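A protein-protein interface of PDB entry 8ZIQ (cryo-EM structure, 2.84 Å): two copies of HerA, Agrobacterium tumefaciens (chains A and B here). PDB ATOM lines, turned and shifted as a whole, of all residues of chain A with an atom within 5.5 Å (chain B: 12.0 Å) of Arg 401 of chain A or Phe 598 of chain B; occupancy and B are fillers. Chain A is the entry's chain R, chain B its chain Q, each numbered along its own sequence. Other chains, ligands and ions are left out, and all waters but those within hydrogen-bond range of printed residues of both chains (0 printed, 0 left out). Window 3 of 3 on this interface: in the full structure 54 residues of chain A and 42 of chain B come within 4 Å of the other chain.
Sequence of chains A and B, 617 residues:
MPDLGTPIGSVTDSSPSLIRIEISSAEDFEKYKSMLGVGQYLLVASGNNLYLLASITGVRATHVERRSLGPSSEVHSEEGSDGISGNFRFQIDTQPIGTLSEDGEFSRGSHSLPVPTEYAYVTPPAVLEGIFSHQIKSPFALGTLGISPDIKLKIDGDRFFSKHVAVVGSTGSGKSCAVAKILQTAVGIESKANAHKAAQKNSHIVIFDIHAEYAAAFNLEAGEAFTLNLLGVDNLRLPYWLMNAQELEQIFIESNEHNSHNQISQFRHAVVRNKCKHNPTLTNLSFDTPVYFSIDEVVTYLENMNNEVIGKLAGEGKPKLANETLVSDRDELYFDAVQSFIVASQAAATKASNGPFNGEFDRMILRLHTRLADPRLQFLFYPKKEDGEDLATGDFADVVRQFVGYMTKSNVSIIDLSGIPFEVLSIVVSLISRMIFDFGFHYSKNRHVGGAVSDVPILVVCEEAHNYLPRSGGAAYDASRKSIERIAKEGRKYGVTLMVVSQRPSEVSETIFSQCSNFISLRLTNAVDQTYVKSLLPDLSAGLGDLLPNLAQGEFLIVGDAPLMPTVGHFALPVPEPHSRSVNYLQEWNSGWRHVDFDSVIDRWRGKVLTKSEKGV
Ile 602 of chain B touches Ala 397 of chain A (CG1 to CB, 3.9 Å).
CE1 of Phe 598 of chain B touches CG1 of Val 400 of chain A (3.7 Å).
CB of Phe 598 of chain B touches NH1 of Arg 401 of chain A, 3.9 Å away.
Tyr 406 of chain A touches Trp 593 of chain B.
Arg 594 of chain B touches Tyr 406 of chain A (O to CE1, 3.6 Å).
Val 596 of chain B touches Tyr 406 of chain A.
CE2 of Phe 598 of chain B touches CB of Tyr 406 of chain A (3.2 Å).
Phe 439 of chain A touches Phe 598 of chain B.
Trp 605 of chain B touches Phe 439 of chain A (CZ3 to N, 3.96 Å).
The backbone carbonyl oxygen of Arg 401 of chain A lies within hydrogen-bond range of the backbone NH of Met 407 of chain A, at 3.4 Å.
The backbone carbonyl oxygen (O) of Arg 401 of chain A is in hydrogen-bond range of the backbone NH (N) of Tyr 406 of chain A (3.4 Å).
Asp 398 of chain A touches none of the printed residues of chain B.
No residue of chain B comes within 4 Å of Val 399 of chain A.
No residue of chain B comes within 4 Å of Gln 402 of chain A.
No residue of chain B comes within 4 Å of Phe 403 of chain A.
Val 404 of chain A touches none of the printed residues of chain B.
Tyr 406 of chain A touches four residues of chain B.
Of the printed residues of chain B, Phe 439 of chain A touches Phe 598 (3.4 Å) and Trp 605 (3.96 Å).
Printed residues of chain A within 4 Å of Trp 593 of chain B: Tyr 406.
Printed residues of chain A within 4 Å of Arg 594 of chain B: Tyr 406.
Of the printed residues of chain A, Val 596 of chain B touches Tyr 406.
Phe 598 of chain B touches just these residues of chain A: Val 400 (3.7 Å), Arg 401 (3.9 Å), Tyr 406 (3.2 Å) and Phe 439 (3.4 Å).
Ser 600 of chain B touches none of the printed residues of chain A.
Of the printed residues of chain A, Trp 605 of chain B touches Phe 439.
The nearest printed residue of chain B that does not touch Phe 439 of chain A is Val 596 of chain B (4.3 Å).
Printed residues of chain A that touch a printed residue of chain B: Ala 397, Val 400, Arg 401, Tyr 406 and Phe 439.
Hydrophobic or aromatic side chains of chain A within 4 Å of the printed part of chain B: Ala 397, Val 400, Tyr 406 and Phe 439.
Hydrophobic or aromatic side chains of chain B within 4 Å of the printed part of chain A: Trp 593, Val 596, Phe 598, Ile 602 and Trp 605.
Among the printed residues, no Asp or Glu carboxylate lies within 4 Å of a Lys or Arg side-chain nitrogen of the other chain.
No position is printed for both chains.
Of the 9 pairs that touch across the chains among the printed residues, none has its exchanged pair printed and touching as well.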
ATOM      1  N   ALA A 397      -2.243  16.946   5.502  1.00  0.00           N
ATOM      2  CA  ALA A 397      -2.349  16.376   4.172  1.00  0.00           C
ATOM      3  C   ALA A 397      -1.366  17.034   3.223  1.00  0.00           C
ATOM      4  O   ALA A 397      -0.811  16.379   2.333  1.00  0.00           O
ATOM      5  CB  ALA A 397      -3.776  16.530   3.652  1.00  0.00           C
ATOM      6  N   ASP A 398      -1.135  18.332   3.402  1.00  0.00           N
ATOM      7  CA  ASP A 398      -0.320  19.073   2.455  1.00  0.00           C
ATOM      8  C   ASP A 398       1.013  18.389   2.258  1.00  0.00           C
ATOM      9  O   ASP A 398       1.527  18.316   1.137  1.00  0.00           O
ATOM     10  CB  ASP A 398      -0.109  20.501   2.945  1.00  0.00           C
ATOM     11  CG  ASP A 398       0.605  21.363   1.925  1.00  0.00           C
ATOM     12  OD1 ASP A 398       0.827  20.881   0.794  1.00  0.00           O
ATOM     13  OD2 ASP A 398       0.945  22.520   2.252  1.00  0.00           O
ATOM     14  N   VAL A 399       1.557  17.817   3.325  1.00  0.00           N
ATOM     15  CA  VAL A 399       2.884  17.239   3.222  1.00  0.00           C
ATOM     16  C   VAL A 399       2.843  16.038   2.286  1.00  0.00           C
ATOM     17  O   VAL A 399       3.652  15.919   1.357  1.00  0.00           O
ATOM     18  CB  VAL A 399       3.401  16.860   4.619  1.00  0.00           C
ATOM     19  CG1 VAL A 399       4.821  16.393   4.551  1.00  0.00           C
ATOM     20  CG2 VAL A 399       3.290  18.014   5.552  1.00  0.00           C
ATOM     21  N   VAL A 400       1.836  15.180   2.464  1.00  0.00           N
ATOM     22  CA  VAL A 400       1.633  14.055   1.559  1.00  0.00           C
ATOM     23  C   VAL A 400       1.389  14.541   0.146  1.00  0.00           C
ATOM     24  O   VAL A 400       1.790  13.890  -0.824  1.00  0.00           O
ATOM     25  CB  VAL A 400       0.451  13.200   2.040  1.00  0.00           C
ATOM     26  CG1 VAL A 400      -0.059  12.333   0.925  1.00  0.00           C
ATOM     27  CG2 VAL A 400       0.838  12.379   3.222  1.00  0.00           C
ATOM     28  N   ARG A 401       0.739  15.692   0.003  1.00  0.00           N
ATOM     29  CA  ARG A 401       0.468  16.213  -1.325  1.00  0.00           C
ATOM     30  C   ARG A 401       1.758  16.487  -2.067  1.00  0.00           C
ATOM     31  O   ARG A 401       1.803  16.399  -3.297  1.00  0.00           O
ATOM     32  CB  ARG A 401      -0.373  17.476  -1.229  1.00  0.00           C
ATOM     33  CG  ARG A 401      -1.863  17.233  -1.093  1.00  0.00           C
ATOM     34  CD  ARG A 401      -2.570  18.545  -0.780  1.00  0.00           C
ATOM     35  NE  ARG A 401      -3.776  18.383   0.029  1.00  0.00           N
ATOM     36  CZ  ARG A 401      -5.000  18.745  -0.340  1.00  0.00           C
ATOM     37  NH1 ARG A 401      -6.013  18.546   0.483  1.00  0.00           N
ATOM     38  NH2 ARG A 401      -5.222  19.291  -1.524  1.00  0.00           N
ATOM     39  N   GLN A 402       2.813  16.819  -1.340  1.00  0.00           N
ATOM     40  CA  GLN A 402       4.021  17.326  -1.963  1.00  0.00           C
ATOM     41  C   GLN A 402       4.792  16.203  -2.637  1.00  0.00           C
ATOM     42  O   GLN A 402       5.124  16.290  -3.823  1.00  0.00           O
ATOM     43  CB  GLN A 402       4.865  18.014  -0.903  1.00  0.00           C
ATOM     44  CG  GLN A 402       6.106  18.693  -1.399  1.00  0.00           C
ATOM     45  CD  GLN A 402       6.833  19.410  -0.276  1.00  0.00           C
ATOM     46  OE1 GLN A 402       6.571  19.164   0.902  1.00  0.00           O
ATOM     47  NE2 GLN A 402       7.725  20.321  -0.633  1.00  0.00           N
ATOM     48  N   PHE A 403       5.106  15.152  -1.884  1.00  0.00           N
ATOM     49  CA  PHE A 403       6.007  14.120  -2.373  1.00  0.00           C
ATOM     50  C   PHE A 403       5.359  13.287  -3.468  1.00  0.00           C
ATOM     51  O   PHE A 403       6.069  12.709  -4.297  1.00  0.00           O
ATOM     52  CB  PHE A 403       6.437  13.239  -1.211  1.00  0.00           C
ATOM     53  CG  PHE A 403       7.136  13.986  -0.115  1.00  0.00           C
ATOM     54  CD1 PHE A 403       7.971  15.050  -0.396  1.00  0.00           C
ATOM     55  CD2 PHE A 403       6.931  13.638   1.205  1.00  0.00           C
ATOM     56  CE1 PHE A 403       8.606  15.740   0.622  1.00  0.00           C
ATOM     57  CE2 PHE A 403       7.558  14.319   2.224  1.00  0.00           C
ATOM     58  CZ  PHE A 403       8.393  15.376   1.935  1.00  0.00           C
ATOM     59  N   VAL A 404       4.028  13.218  -3.487  1.00  0.00           N
ATOM     60  CA  VAL A 404       3.312  12.431  -4.485  1.00  0.00           C
ATOM     61  C   VAL A 404       3.160  13.208  -5.782  1.00  0.00           C
ATOM     62  O   VAL A 404       3.375  12.670  -6.872  1.00  0.00           O
ATOM     63  CB  VAL A 404       1.950  11.997  -3.926  1.00  0.00           C
ATOM     64  CG1 VAL A 404       1.177  11.268  -4.951  1.00  0.00           C
ATOM     65  CG2 VAL A 404       2.133  11.118  -2.713  1.00  0.00           C
ATOM     66  N   GLY A 405       2.775  14.475  -5.688  1.00  0.00           N
ATOM     67  CA  GLY A 405       2.668  15.324  -6.854  1.00  0.00           C
ATOM     68  C   GLY A 405       1.292  15.870  -7.151  1.00  0.00           C
ATOM     69  O   GLY A 405       1.091  16.504  -8.191  1.00  0.00           O
ATOM     70  N   TYR A 406       0.338  15.644  -6.257  1.00  0.00           N
ATOM     71  CA  TYR A 406      -1.002  16.170  -6.451  1.00  0.00           C
ATOM     72  C   TYR A 406      -1.151  17.625  -6.017  1.00  0.00           C
ATOM     73  O   TYR A 406      -2.202  18.222  -6.276  1.00  0.00           O
ATOM     74  CB  TYR A 406      -1.994  15.309  -5.685  1.00  0.00           C
ATOM     75  CG  TYR A 406      -2.265  13.963  -6.301  1.00  0.00           C
ATOM     76  CD1 TYR A 406      -3.200  13.816  -7.311  1.00  0.00           C
ATOM     77  CD2 TYR A 406      -1.588  12.838  -5.871  1.00  0.00           C
ATOM     78  CE1 TYR A 406      -3.454  12.593  -7.871  1.00  0.00           C
ATOM     79  CE2 TYR A 406      -1.835  11.603  -6.431  1.00  0.00           C
ATOM     80  CZ  TYR A 406      -2.768  11.492  -7.436  1.00  0.00           C
ATOM     81  OH  TYR A 406      -3.029  10.266  -7.998  1.00  0.00           O
ATOM     82  N   MET A 407      -0.141  18.209  -5.367  1.00  0.00           N
ATOM     83  CA  MET A 407      -0.230  19.611  -4.967  1.00  0.00           C
ATOM     84  C   MET A 407      -0.158  20.550  -6.165  1.00  0.00           C
ATOM     85  O   MET A 407      -0.949  21.494  -6.276  1.00  0.00           O
ATOM     86  CB  MET A 407       0.880  19.947  -3.976  1.00  0.00           C
ATOM     87  CG  MET A 407       0.732  21.315  -3.361  1.00  0.00           C
ATOM     88  SD  MET A 407      -0.707  21.435  -2.285  1.00  0.00           S
ATOM     89  CE  MET A 407      -1.018  23.196  -2.350  1.00  0.00           C
ATOM     90  N   PHE A 439       0.271   5.844   2.443  1.00  0.00           N
ATOM     91  CA  PHE A 439      -0.741   6.492   1.624  1.00  0.00           C
ATOM     92  C   PHE A 439      -1.464   5.464   0.779  1.00  0.00           C
ATOM     93  O   PHE A 439      -2.699   5.385   0.780  1.00  0.00           O
ATOM     94  CB  PHE A 439      -0.086   7.553   0.753  1.00  0.00           C
ATOM     95  CG  PHE A 439      -0.961   8.083  -0.330  1.00  0.00           C
ATOM     96  CD1 PHE A 439      -1.050   7.453  -1.539  1.00  0.00           C
ATOM     97  CD2 PHE A 439      -1.684   9.234  -0.135  1.00  0.00           C
ATOM     98  CE1 PHE A 439      -1.846   7.954  -2.530  1.00  0.00           C
ATOM     99  CE2 PHE A 439      -2.482   9.729  -1.126  1.00  0.00           C
ATOM    100  CZ  PHE A 439      -2.562   9.078  -2.323  1.00  0.00           C
ATOM    101  N   TRP B 593      -5.616  11.894 -15.366  1.00  0.00           N
ATOM    102  CA  TRP B 593      -5.569  12.253 -13.958  1.00  0.00           C
ATOM    103  C   TRP B 593      -6.849  11.852 -13.250  1.00  0.00           C
ATOM    104  O   TRP B 593      -7.929  11.811 -13.844  1.00  0.00           O
ATOM    105  CB  TRP B 593      -5.350  13.746 -13.813  1.00  0.00           C
ATOM    106  CG  TRP B 593      -4.471  14.097 -12.703  1.00  0.00           C
ATOM    107  CD1 TRP B 593      -4.831  14.577 -11.491  1.00  0.00           C
ATOM    108  CD2 TRP B 593      -3.055  14.008 -12.700  1.00  0.00           C
ATOM    109  NE1 TRP B 593      -3.721  14.796 -10.722  1.00  0.00           N
ATOM    110  CE2 TRP B 593      -2.613  14.452 -11.445  1.00  0.00           C
ATOM    111  CE3 TRP B 593      -2.113  13.594 -13.638  1.00  0.00           C
ATOM    112  CZ2 TRP B 593      -1.277  14.492 -11.104  1.00  0.00           C
ATOM    113  CZ3 TRP B 593      -0.790  13.631 -13.300  1.00  0.00           C
ATOM    114  CH2 TRP B 593      -0.377  14.078 -12.043  1.00  0.00           C
ATOM    115  N   ARG B 594      -6.721  11.547 -11.963  1.00  0.00           N
ATOM    116  CA  ARG B 594      -7.861  11.174 -11.141  1.00  0.00           C
ATOM    117  C   ARG B 594      -7.801  11.994  -9.867  1.00  0.00           C
ATOM    118  O   ARG B 594      -6.809  11.925  -9.136  1.00  0.00           O
ATOM    119  CB  ARG B 594      -7.841   9.681 -10.813  1.00  0.00           C
ATOM    120  CG  ARG B 594      -8.150   8.787 -11.996  1.00  0.00           C
ATOM    121  CD  ARG B 594      -8.241   7.333 -11.585  1.00  0.00           C
ATOM    122  NE  ARG B 594      -8.389   6.444 -12.735  1.00  0.00           N
ATOM    123  CZ  ARG B 594      -9.549   6.070 -13.269  1.00  0.00           C
ATOM    124  NH1 ARG B 594     -10.699   6.497 -12.762  1.00  0.00           N
ATOM    125  NH2 ARG B 594      -9.556   5.255 -14.314  1.00  0.00           N
ATOM    126  N   HIS B 595      -8.838  12.780  -9.610  1.00  0.00           N
ATOM    127  CA  HIS B 595      -8.890  13.550  -8.380  1.00  0.00           C
ATOM    128  C   HIS B 595      -8.812  12.636  -7.167  1.00  0.00           C
ATOM    129  O   HIS B 595      -9.510  11.623  -7.090  1.00  0.00           O
ATOM    130  CB  HIS B 595     -10.150  14.405  -8.331  1.00  0.00           C
ATOM    131  CG  HIS B 595     -11.418  13.620  -8.254  1.00  0.00           C
ATOM    132  ND1 HIS B 595     -12.008  13.046  -9.359  1.00  0.00           N
ATOM    133  CD2 HIS B 595     -12.215  13.319  -7.202  1.00  0.00           C
ATOM    134  CE1 HIS B 595     -13.113  12.423  -8.990  1.00  0.00           C
ATOM    135  NE2 HIS B 595     -13.261  12.574  -7.686  1.00  0.00           N
ATOM    136  N   VAL B 596      -7.939  13.001  -6.232  1.00  0.00           N
ATOM    137  CA  VAL B 596      -7.689  12.267  -4.997  1.00  0.00           C
ATOM    138  C   VAL B 596      -8.221  13.097  -3.848  1.00  0.00           C
ATOM    139  O   VAL B 596      -7.666  14.143  -3.505  1.00  0.00           O
ATOM    140  CB  VAL B 596      -6.213  11.893  -4.824  1.00  0.00           C
ATOM    141  CG1 VAL B 596      -6.021  11.348  -3.419  1.00  0.00           C
ATOM    142  CG2 VAL B 596      -5.776  10.903  -5.893  1.00  0.00           C
ATOM    143  N   ASP B 597      -9.273  12.591  -3.216  1.00  0.00           N
ATOM    144  CA  ASP B 597      -9.918  13.273  -2.109  1.00  0.00           C
ATOM    145  C   ASP B 597      -9.038  13.048  -0.885  1.00  0.00           C
ATOM    146  O   ASP B 597      -9.345  12.266   0.015  1.00  0.00           O
ATOM    147  CB  ASP B 597     -11.338  12.771  -1.921  1.00  0.00           C
ATOM    148  CG  ASP B 597     -12.113  13.619  -0.948  1.00  0.00           C
ATOM    149  OD1 ASP B 597     -11.564  14.652  -0.514  1.00  0.00           O
ATOM    150  OD2 ASP B 597     -13.264  13.269  -0.628  1.00  0.00           O
ATOM    151  N   PHE B 598      -7.938  13.794  -0.850  1.00  0.00           N
ATOM    152  CA  PHE B 598      -6.927  13.611   0.184  1.00  0.00           C
ATOM    153  C   PHE B 598      -7.521  13.693   1.584  1.00  0.00           C
ATOM    154  O   PHE B 598      -7.099  12.960   2.486  1.00  0.00           O
ATOM    155  CB  PHE B 598      -5.839  14.666   0.025  1.00  0.00           C
ATOM    156  CG  PHE B 598      -4.771  14.296  -0.961  1.00  0.00           C
ATOM    157  CD1 PHE B 598      -3.727  13.472  -0.599  1.00  0.00           C
ATOM    158  CD2 PHE B 598      -4.815  14.783  -2.255  1.00  0.00           C
ATOM    159  CE1 PHE B 598      -2.747  13.134  -1.507  1.00  0.00           C
ATOM    160  CE2 PHE B 598      -3.839  14.448  -3.166  1.00  0.00           C
ATOM    161  CZ  PHE B 598      -2.802  13.625  -2.790  1.00  0.00           C
ATOM    162  N   ASP B 599      -8.484  14.585   1.794  1.00  0.00           N
ATOM    163  CA  ASP B 599      -9.019  14.770   3.139  1.00  0.00           C
ATOM    164  C   ASP B 599      -9.574  13.465   3.688  1.00  0.00           C
ATOM    165  O   ASP B 599      -9.355  13.127   4.855  1.00  0.00           O
ATOM    166  CB  ASP B 599     -10.106  15.845   3.127  1.00  0.00           C
ATOM    167  CG  ASP B 599     -11.310  15.449   2.288  1.00  0.00           C
ATOM    168  OD1 ASP B 599     -12.245  16.267   2.153  1.00  0.00           O
ATOM    169  OD2 ASP B 599     -11.342  14.301   1.801  1.00  0.00           O
ATOM    170  N   SER B 600     -10.300  12.720   2.861  1.00  0.00           N
ATOM    171  CA  SER B 600     -10.917  11.484   3.321  1.00  0.00           C
ATOM    172  C   SER B 600      -9.867  10.433   3.658  1.00  0.00           C
ATOM    173  O   SER B 600      -9.919   9.804   4.723  1.00  0.00           O
ATOM    174  CB  SER B 600     -11.886  10.974   2.265  1.00  0.00           C
ATOM    175  OG  SER B 600     -11.217  10.643   1.065  1.00  0.00           O
ATOM    176  N   VAL B 601      -8.940  10.184   2.732  1.00  0.00           N
ATOM    177  CA  VAL B 601      -7.917   9.175   2.975  1.00  0.00           C
ATOM    178  C   VAL B 601      -7.177   9.518   4.251  1.00  0.00           C
ATOM    179  O   VAL B 601      -6.838   8.638   5.052  1.00  0.00           O
ATOM    180  CB  VAL B 601      -6.958   9.043   1.779  1.00  0.00           C
ATOM    181  CG1 VAL B 601      -7.675   8.420   0.593  1.00  0.00           C
ATOM    182  CG2 VAL B 601      -6.356  10.374   1.408  1.00  0.00           C
ATOM    183  N   ILE B 602      -6.922  10.805   4.465  1.00  0.00           N
ATOM    184  CA  ILE B 602      -6.163  11.217   5.634  1.00  0.00           C
ATOM    185  C   ILE B 602      -7.000  11.019   6.884  1.00  0.00           C
ATOM    186  O   ILE B 602      -6.492  10.593   7.926  1.00  0.00           O
ATOM    187  CB  ILE B 602      -5.703  12.678   5.491  1.00  0.00           C
ATOM    188  CG1 ILE B 602      -4.676  12.824   4.365  1.00  0.00           C
ATOM    189  CG2 ILE B 602      -5.169  13.193   6.812  1.00  0.00           C
ATOM    190  CD1 ILE B 602      -3.394  12.039   4.565  1.00  0.00           C
ATOM    191  N   ASP B 603      -8.298  11.304   6.802  1.00  0.00           N
ATOM    192  CA  ASP B 603      -9.167  11.090   7.950  1.00  0.00           C
ATOM    193  C   ASP B 603      -9.148   9.630   8.367  1.00  0.00           C
ATOM    194  O   ASP B 603      -9.011   9.310   9.553  1.00  0.00           O
ATOM    195  CB  ASP B 603     -10.588  11.534   7.619  1.00  0.00           C
ATOM    196  CG  ASP B 603     -11.325  12.073   8.828  1.00  0.00           C
ATOM    197  OD1 ASP B 603     -12.392  12.698   8.651  1.00  0.00           O
ATOM    198  OD2 ASP B 603     -10.837  11.868   9.960  1.00  0.00           O
ATOM    199  N   ARG B 604      -9.292   8.724   7.402  1.00  0.00           N
ATOM    200  CA  ARG B 604      -9.195   7.305   7.733  1.00  0.00           C
ATOM    201  C   ARG B 604      -7.828   6.985   8.324  1.00  0.00           C
ATOM    202  O   ARG B 604      -7.719   6.213   9.283  1.00  0.00           O
ATOM    203  CB  ARG B 604      -9.439   6.441   6.498  1.00  0.00           C
ATOM    204  CG  ARG B 604      -9.348   4.938   6.778  1.00  0.00           C
ATOM    205  CD  ARG B 604     -10.055   4.107   5.715  1.00  0.00           C
ATOM    206  NE  ARG B 604     -10.274   2.726   6.134  1.00  0.00           N
ATOM    207  CZ  ARG B 604     -11.378   2.276   6.723  1.00  0.00           C
ATOM    208  NH1 ARG B 604     -12.396   3.089   6.974  1.00  0.00           N
ATOM    209  NH2 ARG B 604     -11.463   0.997   7.064  1.00  0.00           N
ATOM    210  N   TRP B 605      -6.772   7.549   7.740  1.00  0.00           N
ATOM    211  CA  TRP B 605      -5.430   7.352   8.262  1.00  0.00           C
ATOM    212  C   TRP B 605      -5.363   7.691   9.740  1.00  0.00           C
ATOM    213  O   TRP B 605      -4.671   7.012  10.505  1.00  0.00           O
ATOM    214  CB  TRP B 605      -4.463   8.245   7.489  1.00  0.00           C
ATOM    215  CG  TRP B 605      -3.003   8.011   7.720  1.00  0.00           C
ATOM    216  CD1 TRP B 605      -2.409   7.586   8.855  1.00  0.00           C
ATOM    217  CD2 TRP B 605      -1.949   8.264   6.790  1.00  0.00           C
ATOM    218  NE1 TRP B 605      -1.056   7.535   8.694  1.00  0.00           N
ATOM    219  CE2 TRP B 605      -0.747   7.947   7.428  1.00  0.00           C
ATOM    220  CE3 TRP B 605      -1.910   8.718   5.472  1.00  0.00           C
ATOM    221  CZ2 TRP B 605       0.480   8.065   6.800  1.00  0.00           C
ATOM    222  CZ3 TRP B 605      -0.699   8.829   4.853  1.00  0.00           C
ATOM    223  CH2 TRP B 605       0.480   8.509   5.512  1.00  0.00           C
ATOM    224  N   ARG B 606      -6.126   8.699  10.168  1.00  0.00           N
ATOM    225  CA  ARG B 606      -5.975   9.240  11.516  1.00  0.00           C
ATOM    226  C   ARG B 606      -6.028   8.161  12.579  1.00  0.00           C
ATOM    227  O   ARG B 606      -5.230   8.169  13.523  1.00  0.00           O
ATOM    228  CB  ARG B 606      -7.069  10.263  11.801  1.00  0.00           C
ATOM    229  CG  ARG B 606      -7.024  11.524  10.959  1.00  0.00           C
ATOM    230  CD  ARG B 606      -6.033  12.543  11.518  1.00  0.00           C
ATOM    231  NE  ARG B 606      -4.646  12.088  11.471  1.00  0.00           N
ATOM    232  CZ  ARG B 606      -3.620  12.776  11.965  1.00  0.00           C
ATOM    233  NH1 ARG B 606      -3.821  13.947  12.558  1.00  0.00           N
ATOM    234  NH2 ARG B 606      -2.390  12.288  11.879  1.00  0.00           N
ATOM    235  N   GLY B 607      -6.945   7.227  12.443  1.00  0.00           N
ATOM    236  CA  GLY B 607      -7.140   6.263  13.491  1.00  0.00           C
ATOM    237  C   GLY B 607      -8.132   6.817  14.488  1.00  0.00           C
ATOM    238  O   GLY B 607      -8.769   7.851  14.268  1.00  0.00           O
